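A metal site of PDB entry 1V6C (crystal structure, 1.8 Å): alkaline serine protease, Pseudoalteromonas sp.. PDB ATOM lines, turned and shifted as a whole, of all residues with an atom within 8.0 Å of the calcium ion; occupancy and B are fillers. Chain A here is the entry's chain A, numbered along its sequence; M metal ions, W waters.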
ATOM      1  N   ASP A 403     -29.397 -20.016  16.928  1.00  0.00           N
ATOM      2  CA  ASP A 403     -29.546 -18.604  16.602  1.00  0.00           C
ATOM      3  C   ASP A 403     -29.083 -17.747  17.759  1.00  0.00           C
ATOM      4  O   ASP A 403     -29.685 -17.736  18.832  1.00  0.00           O
ATOM      5  CB  ASP A 403     -31.013 -18.288  16.264  1.00  0.00           C
ATOM      6  CG  ASP A 403     -31.508 -19.049  15.042  1.00  0.00           C
ATOM      7  OD1 ASP A 403     -30.823 -19.011  13.991  1.00  0.00           O
ATOM      8  OD2 ASP A 403     -32.572 -19.688  15.126  1.00  0.00           O
ATOM      9  N   ASP A 404     -27.985 -17.028  17.530  1.00  0.00           N
ATOM     10  CA  ASP A 404     -27.384 -16.154  18.541  1.00  0.00           C
ATOM     11  C   ASP A 404     -28.408 -15.196  19.138  1.00  0.00           C
ATOM     12  O   ASP A 404     -29.104 -14.479  18.415  1.00  0.00           O
ATOM     13  CB  ASP A 404     -26.227 -15.383  17.912  1.00  0.00           C
ATOM     14  CG  ASP A 404     -25.345 -14.692  18.940  1.00  0.00           C
ATOM     15  OD1 ASP A 404     -25.520 -14.945  20.149  1.00  0.00           O
ATOM     16  OD2 ASP A 404     -24.462 -13.909  18.525  1.00  0.00           O
ATOM     17  N   LEU A 405     -28.502 -15.190  20.469  1.00  0.00           N
ATOM     18  CA  LEU A 405     -29.431 -14.323  21.185  1.00  0.00           C
ATOM     19  C   LEU A 405     -28.669 -13.345  22.078  1.00  0.00           C
ATOM     20  O   LEU A 405     -27.462 -13.485  22.277  1.00  0.00           O
ATOM     21  CB  LEU A 405     -30.369 -15.147  22.069  1.00  0.00           C
ATOM     22  CG  LEU A 405     -31.193 -16.274  21.427  1.00  0.00           C
ATOM     23  CD1 LEU A 405     -32.058 -16.926  22.507  1.00  0.00           C
ATOM     24  CD2 LEU A 405     -32.076 -15.712  20.309  1.00  0.00           C
ATOM     25  N   SER A 406     -29.383 -12.362  22.620  1.00  0.00           N
ATOM     26  CA  SER A 406     -28.769 -11.382  23.513  1.00  0.00           C
ATOM     27  C   SER A 406     -27.511 -10.780  22.877  1.00  0.00           C
ATOM     28  O   SER A 406     -27.483 -10.519  21.676  1.00  0.00           O
ATOM     29  CB  SER A 406     -28.426 -12.046  24.848  1.00  0.00           C
ATOM     30  OG  SER A 406     -28.000 -11.099  25.811  1.00  0.00           O
ATOM     31  N   VAL A 407     -26.485 -10.555  23.679  1.00  0.00           N
ATOM     32  CA  VAL A 407     -25.242  -9.983  23.180  1.00  0.00           C
ATOM     33  C   VAL A 407     -24.590 -10.918  22.167  1.00  0.00           C
ATOM     34  O   VAL A 407     -24.702 -12.144  22.264  1.00  0.00           O
ATOM     35  CB  VAL A 407     -24.253  -9.695  24.346  1.00  0.00           C
ATOM     36  CG1 VAL A 407     -23.876 -11.002  25.037  1.00  0.00           C
ATOM     37  CG2 VAL A 407     -23.019  -8.983  23.818  1.00  0.00           C
ATOM     38  N   ALA A 408     -23.890 -10.341  21.196  1.00  0.00           N
ATOM     39  CA  ALA A 408     -23.220 -11.118  20.168  1.00  0.00           C
ATOM     40  C   ALA A 408     -22.280 -12.161  20.757  1.00  0.00           C
ATOM     41  O   ALA A 408     -21.546 -11.881  21.717  1.00  0.00           O
ATOM     42  CB  ALA A 408     -22.436 -10.179  19.235  1.00  0.00           C
ATOM     43  N   GLY A 409     -22.313 -13.359  20.186  1.00  0.00           N
ATOM     44  CA  GLY A 409     -21.459 -14.432  20.656  1.00  0.00           C
ATOM     45  C   GLY A 409     -22.055 -15.217  21.809  1.00  0.00           C
ATOM     46  O   GLY A 409     -23.135 -14.870  22.307  1.00  0.00           O
ATOM     47  N   ARG A 410     -21.364 -16.260  22.237  1.00  0.00           N
ATOM     48  CA  ARG A 410     -21.846 -17.069  23.353  1.00  0.00           C
ATOM     49  C   ARG A 410     -21.873 -16.233  24.629  1.00  0.00           C
ATOM     50  O   ARG A 410     -20.943 -15.481  24.905  1.00  0.00           O
ATOM     51  CB  ARG A 410     -20.941 -18.284  23.558  1.00  0.00           C
ATOM     52  CG  ARG A 410     -21.378 -19.210  24.687  1.00  0.00           C
ATOM     53  CD  ARG A 410     -20.451 -20.412  24.832  1.00  0.00           C
ATOM     54  NE  ARG A 410     -20.935 -21.356  25.831  1.00  0.00           N
ATOM     55  CZ  ARG A 410     -20.427 -22.574  26.026  1.00  0.00           C
ATOM     56  NH1 ARG A 410     -20.931 -23.366  26.963  1.00  0.00           N
ATOM     57  NH2 ARG A 410     -19.406 -23.000  25.280  1.00  0.00           N
ATOM     58  N   ASP A 411     -22.959 -16.348  25.396  1.00  0.00           N
ATOM     59  CA  ASP A 411     -23.078 -15.633  26.656  1.00  0.00           C
ATOM     60  C   ASP A 411     -23.623 -16.581  27.722  1.00  0.00           C
ATOM     61  O   ASP A 411     -24.172 -17.628  27.395  1.00  0.00           O
ATOM     62  CB  ASP A 411     -23.983 -14.389  26.509  1.00  0.00           C
ATOM     63  CG  ASP A 411     -25.351 -14.715  25.944  1.00  0.00           C
ATOM     64  OD1 ASP A 411     -25.577 -14.439  24.746  1.00  0.00           O
ATOM     65  OD2 ASP A 411     -26.194 -15.235  26.694  1.00  0.00           O
ATOM     66  N   ASN A 412     -23.438 -16.205  28.984  1.00  0.00           N
ATOM     67  CA  ASN A 412     -23.882 -17.050  30.090  1.00  0.00           C
ATOM     68  C   ASN A 412     -25.391 -17.193  30.246  1.00  0.00           C
ATOM     69  O   ASN A 412     -25.871 -18.141  30.871  1.00  0.00           O
ATOM     70  CB  ASN A 412     -23.292 -16.535  31.409  1.00  0.00           C
ATOM     71  CG  ASN A 412     -21.782 -16.685  31.475  1.00  0.00           C
ATOM     72  OD1 ASN A 412     -21.174 -16.502  32.535  1.00  0.00           O
ATOM     73  ND2 ASN A 412     -21.164 -17.032  30.346  1.00  0.00           N
ATOM     74  N   GLN A 413     -26.140 -16.244  29.689  1.00  0.00           N
ATOM     75  CA  GLN A 413     -27.592 -16.297  29.792  1.00  0.00           C
ATOM     76  C   GLN A 413     -28.243 -17.248  28.795  1.00  0.00           C
ATOM     77  O   GLN A 413     -29.100 -18.056  29.167  1.00  0.00           O
ATOM     78  CB  GLN A 413     -28.182 -14.896  29.600  1.00  0.00           C
ATOM     79  CG  GLN A 413     -28.022 -13.969  30.799  1.00  0.00           C
ATOM     80  CD  GLN A 413     -26.596 -13.486  30.988  1.00  0.00           C
ATOM     81  OE1 GLN A 413     -26.165 -13.237  32.113  1.00  0.00           O
ATOM     82  NE2 GLN A 413     -25.872 -13.344  29.893  1.00  0.00           N
ATOM     83  N   THR A 414     -27.848 -17.159  27.530  1.00  0.00           N
ATOM     84  CA  THR A 414     -28.442 -17.985  26.478  1.00  0.00           C
ATOM     85  C   THR A 414     -27.514 -18.952  25.762  1.00  0.00           C
ATOM     86  O   THR A 414     -27.934 -19.647  24.834  1.00  0.00           O
ATOM     87  CB  THR A 414     -29.094 -17.080  25.425  1.00  0.00           C
ATOM     88  OG1 THR A 414     -28.084 -16.247  24.828  1.00  0.00           O
ATOM     89  CG2 THR A 414     -30.148 -16.189  26.061  1.00  0.00           C
ATOM     90  N   GLY A 415     -26.248 -19.008  26.180  1.00  0.00           N
ATOM     91  CA  GLY A 415     -25.317 -19.905  25.527  1.00  0.00           C
ATOM     92  C   GLY A 415     -25.145 -19.492  24.070  1.00  0.00           C
ATOM     93  O   GLY A 415     -25.042 -18.298  23.774  1.00  0.00           O
ATOM     94  N   TYR A 416     -25.128 -20.458  23.157  1.00  0.00           N
ATOM     95  CA  TYR A 416     -24.975 -20.135  21.740  1.00  0.00           C
ATOM     96  C   TYR A 416     -26.250 -19.569  21.126  1.00  0.00           C
ATOM     97  O   TYR A 416     -26.233 -19.067  20.003  1.00  0.00           O
ATOM     98  CB  TYR A 416     -24.516 -21.367  20.972  1.00  0.00           C
ATOM     99  CG  TYR A 416     -23.068 -21.708  21.230  1.00  0.00           C
ATOM    100  CD1 TYR A 416     -22.039 -20.832  20.860  1.00  0.00           C
ATOM    101  CD2 TYR A 416     -22.720 -22.881  21.890  1.00  0.00           C
ATOM    102  CE1 TYR A 416     -20.708 -21.119  21.145  1.00  0.00           C
ATOM    103  CE2 TYR A 416     -21.387 -23.176  22.181  1.00  0.00           C
ATOM    104  CZ  TYR A 416     -20.391 -22.283  21.809  1.00  0.00           C
ATOM    105  OH  TYR A 416     -19.072 -22.558  22.116  1.00  0.00           O
ATOM    106  N   GLY A 417     -27.359 -19.664  21.859  1.00  0.00           N
ATOM    107  CA  GLY A 417     -28.605 -19.134  21.358  1.00  0.00           C
ATOM    108  C   GLY A 417     -29.752 -20.119  21.285  1.00  0.00           C
ATOM    109  O   GLY A 417     -29.689 -21.208  21.863  1.00  0.00           O
ATOM    110  N   MET A 418     -30.794 -19.739  20.561  1.00  0.00           N
ATOM    111  CA  MET A 418     -31.985 -20.566  20.390  1.00  0.00           C
ATOM    112  C   MET A 418     -31.723 -21.738  19.459  1.00  0.00           C
ATOM    113  O   MET A 418     -31.280 -21.545  18.320  1.00  0.00           O
ATOM    114  CB  MET A 418     -33.138 -19.737  19.840  1.00  0.00           C
ATOM    115  CG  MET A 418     -34.442 -20.498  19.764  1.00  0.00           C
ATOM    116  SD  MET A 418     -35.007 -20.952  21.402  1.00  0.00           S
ATOM    117  CE  MET A 418     -36.710 -20.360  21.370  1.00  0.00           C
HETATM  118 CA    CA M   1     -25.375 -14.349  22.412  1.00  0.00          CA
HETATM  119  O   HOH W   1     -26.601 -16.344  22.637  1.00  0.00           O
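OD2 of Asp 411 is in hydrogen-bond range of N of Thr 414, 2.7 Å away. The side-chain carboxylate (OD2) of Asp 411 lies within hydrogen-bond range of the backbone NH (N) of Gln 413 (3.2 Å).
Of the 16 residues printed, 5 come within 4 Å of the calcium ion.
The backbone carbonyl oxygen (O) of Leu 405 is bound to the calcium ion (2.3 Å). The calcium ion is bound by O of Gly 409. The calcium ion is bound by O of Val 407 (2.3 Å). The side-chain carboxylate (OD1) of Asp 411 binds the calcium ion. OD1 of Asp 404 binds the calcium ion (2.3 Å). The calcium ion is bound by water W1, 2.4 Å away. The calcium ion has six donor atoms within binding distance.
Water W1 lies within hydrogen-bond range of the side-chain hydroxyl (OG1) of Thr 414, the backbone carbonyl oxygen (O) of Gly 415, the backbone NH (N) of Leu 405 and the backbone NH (N) of Gly 417.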
